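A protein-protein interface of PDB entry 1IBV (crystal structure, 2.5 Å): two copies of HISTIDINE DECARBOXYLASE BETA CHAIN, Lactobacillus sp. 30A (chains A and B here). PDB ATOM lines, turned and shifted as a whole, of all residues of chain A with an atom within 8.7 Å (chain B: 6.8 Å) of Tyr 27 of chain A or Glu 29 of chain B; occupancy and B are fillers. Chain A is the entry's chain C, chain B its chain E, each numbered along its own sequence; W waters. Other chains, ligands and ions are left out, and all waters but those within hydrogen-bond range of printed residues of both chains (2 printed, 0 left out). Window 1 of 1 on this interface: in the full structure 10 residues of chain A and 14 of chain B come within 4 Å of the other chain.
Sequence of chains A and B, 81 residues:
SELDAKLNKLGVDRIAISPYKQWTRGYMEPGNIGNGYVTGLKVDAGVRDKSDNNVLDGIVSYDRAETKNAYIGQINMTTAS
Hydrophobic or aromatic side chains of chain B that line the printed part of chain A: Pro 30. Along chain A the printed residues that touch a printed residue of chain B span positions 27 to 35. Among the printed residues, 7 pairs touch across the chains.
The backbone NH of Asn 35 of chain A sits at hydrogen-bond distance from the side-chain carboxylate of Asp 13 of chain A (3.1 Å). The backbone NH (N) of Asn 35 of chain A sits at hydrogen-bond distance from the backbone carbonyl oxygen (O) of Ile 15 of chain A (3.3 Å). The guanidinium group (NE) of Arg 25 of chain B is in salt-bridge range of the side-chain carboxylate (OE1) of Glu 29 of chain B, at 3.9 Å. The guanidinium group (NH2) of Arg 25 of chain B sits at hydrogen-bond distance from the side-chain amide oxygen (OD1) of Asn 32 of chain B (2.8 Å). OE1 of Glu 29 of chain B lies within hydrogen-bond range of N of Gly 26 of chain B, at 2.9 Å. The backbone carbonyl oxygen (O) of Glu 29 of chain B is in hydrogen-bond range of the side-chain amide nitrogen (ND2) of Asn 32 of chain B (3.4 Å).
Water W2 bridges OD1 of Asn 35 of chain A (2.6 Å) and N of Gly 31 of chain B (3.0 Å). Water W1 lies within hydrogen-bond range of the side-chain hydroxyl (OH) of Tyr 20 of chain B, the backbone carbonyl oxygen (O) of Asn 35 of chain A and the backbone carbonyl oxygen (O) of Asp 13 of chain A.
Among the printed residues, pairs that only touch across the chains: Asn 35 of chain A with Gly 31 of chain B (3.5 Å), Tyr 27 of chain A with Pro 30 of chain B (3.5 Å), Asn 35 of chain A with Pro 30 of chain B (3.6 Å), Tyr 27 of chain A with Arg 25 of chain B (3.7 Å), Gly 34 of chain A with Pro 30 of chain B (3.8 Å) and Met 28 of chain A with Met 28 of chain B (3.96 Å).
OH of Tyr 27 of chain A is in hydrogen-bond range of OE2 of Glu 29 of chain B, 2.8 Å away.
Tyr 27 of chain A touches Arg 25 of chain B, but with the chains exchanged Arg 25 of chain A does not touch Tyr 27 of chain B (15.3 Å). Tyr 27 of chain A touches Glu 29 of chain B, but with the chains exchanged Glu 29 of chain A does not touch Tyr 27 of chain B (10.0 Å). Tyr 27 of chain A touches Pro 30 of chain B, but with the chains exchanged Pro 30 of chain A does not touch Tyr 27 of chain B (11.5 Å). Met 28 of chain B touches its own counterpart, Met 28 of chain A. Positions printed for both chains: 24, 25, 26, 27, 28, 29, 30, 32 and 33.
Printed residues of chain B within 4 Å of Tyr 27 of chain A: Arg 25 (3.7 Å), Glu 29 (2.8 Å) and Pro 30 (3.5 Å). Of the printed residues of chain B, Met 28 of chain A touches Met 28. Of the printed residues of chain B, Gly 34 of chain A touches Pro 30. Printed residues of chain B within 4 Å of Asn 35 of chain A: Pro 30 and Gly 31. Val 38 of chain A touches none of the printed residues of chain B. No residue of chain A comes within 4 Å of Gly 26 of chain B. Printed residues of chain A within 4 Å of Met 28 of chain B: Met 28. Of chain A, only Tyr 27 (2.8 Å) comes within 4 Å of Glu 29 of chain B. Of chain A, only Tyr 27 (3.5 Å), Gly 34 (3.8 Å) and Asn 35 (3.6 Å) come within 4 Å of Pro 30 of chain B. Printed residues of chain A within 4 Å of Gly 31 of chain B: Asn 35 (3.5 Å). The nearest residue of chain A that does not touch Glu 29 of chain B is Met 28 of chain A (4.3 Å). The nearest printed residue of chain B that does not touch Asn 35 of chain A is Tyr 20 of chain B (4.03 Å).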
ATOM      1  N   ASP A  13      -1.349   7.231  29.608  1.00  0.00           N
ATOM      2  CA  ASP A  13      -1.577   7.953  30.857  1.00  0.00           C
ATOM      3  C   ASP A  13      -2.696   8.956  30.609  1.00  0.00           C
ATOM      4  O   ASP A  13      -2.782   9.550  29.533  1.00  0.00           O
ATOM      5  CB  ASP A  13      -0.296   8.624  31.403  1.00  0.00           C
ATOM      6  CG  ASP A  13       0.170   9.798  30.571  1.00  0.00           C
ATOM      7  OD1 ASP A  13      -0.349  10.908  30.772  1.00  0.00           O
ATOM      8  OD2 ASP A  13       1.080   9.630  29.743  1.00  0.00           O
ATOM      9  N   ARG A  14      -3.572   9.118  31.587  1.00  0.00           N
ATOM     10  CA  ARG A  14      -4.698  10.021  31.476  1.00  0.00           C
ATOM     11  C   ARG A  14      -4.431  11.336  32.189  1.00  0.00           C
ATOM     12  O   ARG A  14      -5.354  11.986  32.661  1.00  0.00           O
ATOM     13  CB  ARG A  14      -5.945   9.355  32.059  1.00  0.00           C
ATOM     14  CG  ARG A  14      -6.179   7.948  31.552  1.00  0.00           C
ATOM     15  CD  ARG A  14      -7.592   7.474  31.814  1.00  0.00           C
ATOM     16  NE  ARG A  14      -7.820   7.076  33.200  1.00  0.00           N
ATOM     17  CZ  ARG A  14      -9.008   6.714  33.676  1.00  0.00           C
ATOM     18  NH1 ARG A  14      -9.145   6.361  34.946  1.00  0.00           N
ATOM     19  NH2 ARG A  14     -10.061   6.709  32.877  1.00  0.00           N
ATOM     20  N   ILE A  15      -3.162  11.718  32.275  1.00  0.00           N
ATOM     21  CA  ILE A  15      -2.779  12.961  32.934  1.00  0.00           C
ATOM     22  C   ILE A  15      -3.047  14.109  31.983  1.00  0.00           C
ATOM     23  O   ILE A  15      -2.607  14.067  30.844  1.00  0.00           O
ATOM     24  CB  ILE A  15      -1.281  12.973  33.282  1.00  0.00           C
ATOM     25  CG1 ILE A  15      -0.938  11.790  34.176  1.00  0.00           C
ATOM     26  CG2 ILE A  15      -0.905  14.277  33.971  1.00  0.00           C
ATOM     27  CD1 ILE A  15       0.539  11.573  34.328  1.00  0.00           C
ATOM     28  N   ALA A  16      -3.708  15.154  32.463  1.00  0.00           N
ATOM     29  CA  ALA A  16      -4.038  16.315  31.634  1.00  0.00           C
ATOM     30  C   ALA A  16      -4.058  17.591  32.469  1.00  0.00           C
ATOM     31  O   ALA A  16      -5.116  18.027  32.928  1.00  0.00           O
ATOM     32  CB  ALA A  16      -5.388  16.105  30.980  1.00  0.00           C
ATOM     33  N   ILE A  17      -2.899  18.217  32.626  1.00  0.00           N
ATOM     34  CA  ILE A  17      -2.805  19.425  33.436  1.00  0.00           C
ATOM     35  C   ILE A  17      -2.544  20.702  32.644  1.00  0.00           C
ATOM     36  O   ILE A  17      -1.706  20.732  31.748  1.00  0.00           O
ATOM     37  CB  ILE A  17      -1.719  19.260  34.529  1.00  0.00           C
ATOM     38  CG1 ILE A  17      -2.005  18.024  35.389  1.00  0.00           C
ATOM     39  CG2 ILE A  17      -1.646  20.493  35.408  1.00  0.00           C
ATOM     40  CD1 ILE A  17      -3.278  18.123  36.202  1.00  0.00           C
ATOM     41  N   THR A  24      -9.013  26.303  31.835  1.00  0.00           N
ATOM     42  CA  THR A  24      -8.731  24.972  31.323  1.00  0.00           C
ATOM     43  C   THR A  24      -8.148  25.238  29.936  1.00  0.00           C
ATOM     44  O   THR A  24      -8.196  26.374  29.443  1.00  0.00           O
ATOM     45  CB  THR A  24     -10.019  24.147  31.171  1.00  0.00           C
ATOM     46  OG1 THR A  24     -11.124  25.015  30.903  1.00  0.00           O
ATOM     47  CG2 THR A  24     -10.297  23.342  32.415  1.00  0.00           C
ATOM     48  N   ARG A  25      -7.570  24.218  29.315  1.00  0.00           N
ATOM     49  CA  ARG A  25      -7.006  24.356  27.979  1.00  0.00           C
ATOM     50  C   ARG A  25      -7.439  23.134  27.191  1.00  0.00           C
ATOM     51  O   ARG A  25      -7.882  22.146  27.778  1.00  0.00           O
ATOM     52  CB  ARG A  25      -5.480  24.445  28.036  1.00  0.00           C
ATOM     53  CG  ARG A  25      -4.972  25.689  28.734  1.00  0.00           C
ATOM     54  CD  ARG A  25      -3.456  25.751  28.739  1.00  0.00           C
ATOM     55  NE  ARG A  25      -2.909  26.230  27.473  1.00  0.00           N
ATOM     56  CZ  ARG A  25      -1.773  25.793  26.943  1.00  0.00           C
ATOM     57  NH1 ARG A  25      -1.348  26.293  25.797  1.00  0.00           N
ATOM     58  NH2 ARG A  25      -1.083  24.833  27.538  1.00  0.00           N
ATOM     59  N   GLY A  26      -7.299  23.190  25.874  1.00  0.00           N
ATOM     60  CA  GLY A  26      -7.692  22.071  25.046  1.00  0.00           C
ATOM     61  C   GLY A  26      -6.633  20.999  24.898  1.00  0.00           C
ATOM     62  O   GLY A  26      -5.435  21.268  25.015  1.00  0.00           O
ATOM     63  N   TYR A  27      -7.085  19.777  24.645  1.00  0.00           N
ATOM     64  CA  TYR A  27      -6.194  18.656  24.451  1.00  0.00           C
ATOM     65  C   TYR A  27      -5.300  18.994  23.270  1.00  0.00           C
ATOM     66  O   TYR A  27      -5.756  19.568  22.286  1.00  0.00           O
ATOM     67  CB  TYR A  27      -7.004  17.388  24.172  1.00  0.00           C
ATOM     68  CG  TYR A  27      -6.180  16.156  23.827  1.00  0.00           C
ATOM     69  CD1 TYR A  27      -5.199  15.685  24.692  1.00  0.00           C
ATOM     70  CD2 TYR A  27      -6.372  15.477  22.618  1.00  0.00           C
ATOM     71  CE1 TYR A  27      -4.427  14.571  24.361  1.00  0.00           C
ATOM     72  CE2 TYR A  27      -5.604  14.361  22.284  1.00  0.00           C
ATOM     73  CZ  TYR A  27      -4.633  13.917  23.161  1.00  0.00           C
ATOM     74  OH  TYR A  27      -3.847  12.838  22.843  1.00  0.00           O
ATOM     75  N   MET A  28      -4.020  18.665  23.402  1.00  0.00           N
ATOM     76  CA  MET A  28      -2.998  18.907  22.383  1.00  0.00           C
ATOM     77  C   MET A  28      -2.314  20.269  22.396  1.00  0.00           C
ATOM     78  O   MET A  28      -1.306  20.447  21.717  1.00  0.00           O
ATOM     79  CB  MET A  28      -3.524  18.607  20.977  1.00  0.00           C
ATOM     80  CG  MET A  28      -3.830  17.147  20.740  1.00  0.00           C
ATOM     81  SD  MET A  28      -4.261  16.854  19.050  1.00  0.00           S
ATOM     82  CE  MET A  28      -5.944  17.322  19.061  1.00  0.00           C
ATOM     83  N   GLU A  29      -2.850  21.229  23.150  1.00  0.00           N
ATOM     84  CA  GLU A  29      -2.238  22.554  23.218  1.00  0.00           C
ATOM     85  C   GLU A  29      -0.875  22.438  23.891  1.00  0.00           C
ATOM     86  O   GLU A  29      -0.709  21.687  24.858  1.00  0.00           O
ATOM     87  CB  GLU A  29      -3.131  23.532  23.977  1.00  0.00           C
ATOM     88  CG  GLU A  29      -4.458  23.783  23.291  1.00  0.00           C
ATOM     89  CD  GLU A  29      -5.071  25.130  23.629  1.00  0.00           C
ATOM     90  OE1 GLU A  29      -5.649  25.257  24.722  1.00  0.00           O
ATOM     91  OE2 GLU A  29      -4.983  26.061  22.794  1.00  0.00           O
ATOM     92  N   PRO A  30       0.130  23.169  23.383  1.00  0.00           N
ATOM     93  CA  PRO A  30       1.491  23.146  23.925  1.00  0.00           C
ATOM     94  C   PRO A  30       1.558  23.706  25.339  1.00  0.00           C
ATOM     95  O   PRO A  30       0.811  24.618  25.689  1.00  0.00           O
ATOM     96  CB  PRO A  30       2.253  24.021  22.937  1.00  0.00           C
ATOM     97  CG  PRO A  30       1.224  25.024  22.534  1.00  0.00           C
ATOM     98  CD  PRO A  30       0.003  24.179  22.320  1.00  0.00           C
ATOM     99  N   ASN A  32       0.736  22.099  28.022  1.00  0.00           N
ATOM    100  CA  ASN A  32      -0.063  21.227  28.883  1.00  0.00           C
ATOM    101  C   ASN A  32       0.854  20.120  29.357  1.00  0.00           C
ATOM    102  O   ASN A  32       1.757  19.703  28.628  1.00  0.00           O
ATOM    103  CB  ASN A  32      -1.222  20.594  28.117  1.00  0.00           C
ATOM    104  CG  ASN A  32      -2.385  21.531  27.927  1.00  0.00           C
ATOM    105  OD1 ASN A  32      -2.499  22.560  28.589  1.00  0.00           O
ATOM    106  ND2 ASN A  32      -3.267  21.176  27.018  1.00  0.00           N
ATOM    107  N   ILE A  33       0.629  19.638  30.568  1.00  0.00           N
ATOM    108  CA  ILE A  33       1.463  18.584  31.112  1.00  0.00           C
ATOM    109  C   ILE A  33       0.691  17.275  31.122  1.00  0.00           C
ATOM    110  O   ILE A  33      -0.442  17.216  31.606  1.00  0.00           O
ATOM    111  CB  ILE A  33       1.966  18.958  32.531  1.00  0.00           C
ATOM    112  CG1 ILE A  33       2.776  20.250  32.454  1.00  0.00           C
ATOM    113  CG2 ILE A  33       2.842  17.855  33.098  1.00  0.00           C
ATOM    114  CD1 ILE A  33       3.228  20.758  33.776  1.00  0.00           C
ATOM    115  N   GLY A  34       1.292  16.249  30.534  1.00  0.00           N
ATOM    116  CA  GLY A  34       0.662  14.945  30.474  1.00  0.00           C
ATOM    117  C   GLY A  34       0.232  14.596  29.066  1.00  0.00           C
ATOM    118  O   GLY A  34       0.198  15.461  28.191  1.00  0.00           O
ATOM    119  N   ASN A  35      -0.129  13.334  28.859  1.00  0.00           N
ATOM    120  CA  ASN A  35      -0.555  12.853  27.546  1.00  0.00           C
ATOM    121  C   ASN A  35      -1.990  12.315  27.536  1.00  0.00           C
ATOM    122  O   ASN A  35      -2.320  11.433  26.746  1.00  0.00           O
ATOM    123  CB  ASN A  35       0.406  11.766  27.063  1.00  0.00           C
ATOM    124  CG  ASN A  35       1.855  12.188  27.153  1.00  0.00           C
ATOM    125  OD1 ASN A  35       2.175  13.374  27.099  1.00  0.00           O
ATOM    126  ND2 ASN A  35       2.744  11.216  27.297  1.00  0.00           N
ATOM    127  N   GLY A  36      -2.842  12.859  28.394  1.00  0.00           N
ATOM    128  CA  GLY A  36      -4.217  12.405  28.452  1.00  0.00           C
ATOM    129  C   GLY A  36      -5.176  13.561  28.257  1.00  0.00           C
ATOM    130  O   GLY A  36      -4.766  14.648  27.853  1.00  0.00           O
ATOM    131  N   TYR A  37      -6.454  13.331  28.532  1.00  0.00           N
ATOM    132  CA  TYR A  37      -7.454  14.372  28.392  1.00  0.00           C
ATOM    133  C   TYR A  37      -8.657  14.106  29.275  1.00  0.00           C
ATOM    134  O   TYR A  37      -8.855  12.988  29.746  1.00  0.00           O
ATOM    135  CB  TYR A  37      -7.881  14.541  26.924  1.00  0.00           C
ATOM    136  CG  TYR A  37      -8.385  13.279  26.211  1.00  0.00           C
ATOM    137  CD1 TYR A  37      -9.568  12.642  26.602  1.00  0.00           C
ATOM    138  CD2 TYR A  37      -7.683  12.751  25.125  1.00  0.00           C
ATOM    139  CE1 TYR A  37     -10.029  11.518  25.934  1.00  0.00           C
ATOM    140  CE2 TYR A  37      -8.138  11.628  24.449  1.00  0.00           C
ATOM    141  CZ  TYR A  37      -9.309  11.015  24.853  1.00  0.00           C
ATOM    142  OH  TYR A  37      -9.749   9.907  24.165  1.00  0.00           O
ATOM    143  N   VAL A  38      -9.426  15.154  29.536  1.00  0.00           N
ATOM    144  CA  VAL A  38     -10.632  15.069  30.348  1.00  0.00           C
ATOM    145  C   VAL A  38     -11.740  15.638  29.479  1.00  0.00           C
ATOM    146  O   VAL A  38     -11.500  16.566  28.711  1.00  0.00           O
ATOM    147  CB  VAL A  38     -10.508  15.919  31.641  1.00  0.00           C
ATOM    148  CG1 VAL A  38     -11.819  15.922  32.409  1.00  0.00           C
ATOM    149  CG2 VAL A  38      -9.389  15.381  32.528  1.00  0.00           C
ATOM    150  N   THR A  39     -12.938  15.071  29.572  1.00  0.00           N
ATOM    151  CA  THR A  39     -14.069  15.535  28.770  1.00  0.00           C
ATOM    152  C   THR A  39     -15.348  15.672  29.595  1.00  0.00           C
ATOM    153  O   THR A  39     -15.372  15.355  30.790  1.00  0.00           O
ATOM    154  CB  THR A  39     -14.328  14.598  27.576  1.00  0.00           C
ATOM    155  OG1 THR A  39     -15.312  15.177  26.712  1.00  0.00           O
ATOM    156  CG2 THR A  39     -14.823  13.244  28.057  1.00  0.00           C
ATOM    157  N   THR A  78     -12.634  23.216  17.593  1.00  0.00           N
ATOM    158  CA  THR A  78     -12.146  22.354  16.521  1.00  0.00           C
ATOM    159  C   THR A  78     -13.076  21.146  16.532  1.00  0.00           C
ATOM    160  O   THR A  78     -13.498  20.706  17.603  1.00  0.00           O
ATOM    161  CB  THR A  78     -10.710  21.904  16.779  1.00  0.00           C
ATOM    162  OG1 THR A  78      -9.870  23.057  16.919  1.00  0.00           O
ATOM    163  CG2 THR A  78     -10.198  21.061  15.625  1.00  0.00           C
ATOM    164  N   ALA A  80     -14.179  17.147  15.991  1.00  0.00           N
ATOM    165  CA  ALA A  80     -13.790  15.747  15.973  1.00  0.00           C
ATOM    166  C   ALA A  80     -15.091  14.999  15.701  1.00  0.00           C
ATOM    167  O   ALA A  80     -16.123  15.305  16.305  1.00  0.00           O
ATOM    168  CB  ALA A  80     -13.219  15.337  17.309  1.00  0.00           C
ATOM    169  N   TYR B  20       3.023   4.167  22.714  1.00  0.00           N
ATOM    170  CA  TYR B  20       2.116   3.132  23.196  1.00  0.00           C
ATOM    171  C   TYR B  20       2.504   1.733  22.744  1.00  0.00           C
ATOM    172  O   TYR B  20       3.386   1.548  21.908  1.00  0.00           O
ATOM    173  CB  TYR B  20       0.695   3.383  22.696  1.00  0.00           C
ATOM    174  CG  TYR B  20      -0.014   4.596  23.255  1.00  0.00           C
ATOM    175  CD1 TYR B  20       0.556   5.363  24.264  1.00  0.00           C
ATOM    176  CD2 TYR B  20      -1.260   4.979  22.755  1.00  0.00           C
ATOM    177  CE1 TYR B  20      -0.092   6.480  24.763  1.00  0.00           C
ATOM    178  CE2 TYR B  20      -1.914   6.094  23.246  1.00  0.00           C
ATOM    179  CZ  TYR B  20      -1.323   6.838  24.251  1.00  0.00           C
ATOM    180  OH  TYR B  20      -1.956   7.960  24.733  1.00  0.00           O
ATOM    181  N   THR B  24      -1.191   3.011  17.107  1.00  0.00           N
ATOM    182  CA  THR B  24      -0.616   4.163  16.452  1.00  0.00           C
ATOM    183  C   THR B  24      -1.316   5.338  17.120  1.00  0.00           C
ATOM    184  O   THR B  24      -2.285   5.140  17.855  1.00  0.00           O
ATOM    185  CB  THR B  24      -0.938   4.161  14.952  1.00  0.00           C
ATOM    186  OG1 THR B  24      -2.163   3.460  14.726  1.00  0.00           O
ATOM    187  CG2 THR B  24       0.172   3.508  14.161  1.00  0.00           C
ATOM    188  N   ARG B  25      -0.824   6.549  16.898  1.00  0.00           N
ATOM    189  CA  ARG B  25      -1.434   7.734  17.477  1.00  0.00           C
ATOM    190  C   ARG B  25      -1.473   8.787  16.393  1.00  0.00           C
ATOM    191  O   ARG B  25      -0.794   8.658  15.378  1.00  0.00           O
ATOM    192  CB  ARG B  25      -0.625   8.236  18.671  1.00  0.00           C
ATOM    193  CG  ARG B  25      -0.542   7.255  19.822  1.00  0.00           C
ATOM    194  CD  ARG B  25       0.234   7.823  20.994  1.00  0.00           C
ATOM    195  NE  ARG B  25      -0.543   8.798  21.755  1.00  0.00           N
ATOM    196  CZ  ARG B  25      -0.025   9.879  22.331  1.00  0.00           C
ATOM    197  NH1 ARG B  25      -0.810  10.700  23.006  1.00  0.00           N
ATOM    198  NH2 ARG B  25       1.268  10.148  22.211  1.00  0.00           N
ATOM    199  N   GLY B  26      -2.248   9.839  16.608  1.00  0.00           N
ATOM    200  CA  GLY B  26      -2.353  10.886  15.612  1.00  0.00           C
ATOM    201  C   GLY B  26      -1.269  11.941  15.672  1.00  0.00           C
ATOM    202  O   GLY B  26      -0.687  12.200  16.719  1.00  0.00           O
ATOM    203  N   TYR B  27      -1.000  12.554  14.531  1.00  0.00           N
ATOM    204  CA  TYR B  27       0.001  13.601  14.445  1.00  0.00           C
ATOM    205  C   TYR B  27      -0.445  14.692  15.401  1.00  0.00           C
ATOM    206  O   TYR B  27      -1.639  14.967  15.504  1.00  0.00           O
ATOM    207  CB  TYR B  27       0.064  14.140  13.014  1.00  0.00           C
ATOM    208  CG  TYR B  27       0.961  15.340  12.811  1.00  0.00           C
ATOM    209  CD1 TYR B  27       2.309  15.293  13.167  1.00  0.00           C
ATOM    210  CD2 TYR B  27       0.456  16.528  12.273  1.00  0.00           C
ATOM    211  CE1 TYR B  27       3.134  16.402  12.999  1.00  0.00           C
ATOM    212  CE2 TYR B  27       1.273  17.643  12.098  1.00  0.00           C
ATOM    213  CZ  TYR B  27       2.610  17.577  12.467  1.00  0.00           C
ATOM    214  OH  TYR B  27       3.415  18.687  12.340  1.00  0.00           O
ATOM    215  N   MET B  28       0.518  15.269  16.118  1.00  0.00           N
ATOM    216  CA  MET B  28       0.294  16.335  17.095  1.00  0.00           C
ATOM    217  C   MET B  28      -0.106  15.916  18.508  1.00  0.00           C
ATOM    218  O   MET B  28      -0.119  16.744  19.406  1.00  0.00           O
ATOM    219  CB  MET B  28      -0.700  17.374  16.575  1.00  0.00           C
ATOM    220  CG  MET B  28      -0.204  18.153  15.396  1.00  0.00           C
ATOM    221  SD  MET B  28      -1.325  19.462  14.959  1.00  0.00           S
ATOM    222  CE  MET B  28      -2.513  18.554  14.032  1.00  0.00           C
ATOM    223  N   GLU B  29      -0.422  14.644  18.726  1.00  0.00           N
ATOM    224  CA  GLU B  29      -0.806  14.212  20.067  1.00  0.00           C
ATOM    225  C   GLU B  29       0.427  14.271  20.957  1.00  0.00           C
ATOM    226  O   GLU B  29       1.528  13.954  20.510  1.00  0.00           O
ATOM    227  CB  GLU B  29      -1.388  12.793  20.043  1.00  0.00           C
ATOM    228  CG  GLU B  29      -2.682  12.661  19.243  1.00  0.00           C
ATOM    229  CD  GLU B  29      -3.534  11.488  19.681  1.00  0.00           C
ATOM    230  OE1 GLU B  29      -3.220  10.344  19.309  1.00  0.00           O
ATOM    231  OE2 GLU B  29      -4.524  11.706  20.398  1.00  0.00           O
ATOM    232  N   PRO B  30       0.263  14.685  22.227  1.00  0.00           N
ATOM    233  CA  PRO B  30       1.360  14.797  23.191  1.00  0.00           C
ATOM    234  C   PRO B  30       1.949  13.447  23.545  1.00  0.00           C
ATOM    235  O   PRO B  30       1.225  12.464  23.640  1.00  0.00           O
ATOM    236  CB  PRO B  30       0.674  15.417  24.398  1.00  0.00           C
ATOM    237  CG  PRO B  30      -0.683  14.822  24.339  1.00  0.00           C
ATOM    238  CD  PRO B  30      -1.025  14.972  22.881  1.00  0.00           C
ATOM    239  N   GLY B  31       3.253  13.394  23.752  1.00  0.00           N
ATOM    240  CA  GLY B  31       3.888  12.136  24.091  1.00  0.00           C
ATOM    241  C   GLY B  31       4.553  11.486  22.897  1.00  0.00           C
ATOM    242  O   GLY B  31       5.419  10.637  23.062  1.00  0.00           O
ATOM    243  N   ASN B  32       4.128  11.858  21.691  1.00  0.00           N
ATOM    244  CA  ASN B  32       4.716  11.308  20.468  1.00  0.00           C
ATOM    245  C   ASN B  32       6.118  11.859  20.390  1.00  0.00           C
ATOM    246  O   ASN B  32       6.367  12.999  20.797  1.00  0.00           O
ATOM    247  CB  ASN B  32       3.954  11.746  19.211  1.00  0.00           C
ATOM    248  CG  ASN B  32       2.661  10.998  19.019  1.00  0.00           C
ATOM    249  OD1 ASN B  32       2.439   9.952  19.625  1.00  0.00           O
ATOM    250  ND2 ASN B  32       1.791  11.531  18.173  1.00  0.00           N
ATOM    251  N   ILE B  33       7.031  11.069  19.846  1.00  0.00           N
ATOM    252  CA  ILE B  33       8.413  11.487  19.729  1.00  0.00           C
ATOM    253  C   ILE B  33       8.726  11.800  18.286  1.00  0.00           C
ATOM    254  O   ILE B  33       8.539  10.966  17.415  1.00  0.00           O
ATOM    255  CB  ILE B  33       9.352  10.391  20.256  1.00  0.00           C
ATOM    256  CG1 ILE B  33       9.031  10.120  21.728  1.00  0.00           C
ATOM    257  CG2 ILE B  33      10.802  10.809  20.092  1.00  0.00           C
ATOM    258  CD1 ILE B  33       9.765   8.974  22.312  1.00  0.00           C
HETATM  259  O   HOH W   1      -1.364   8.912  27.175  1.00  0.00           O
HETATM  260  O   HOH W   2       4.062  14.969  26.188  1.00  0.00           O
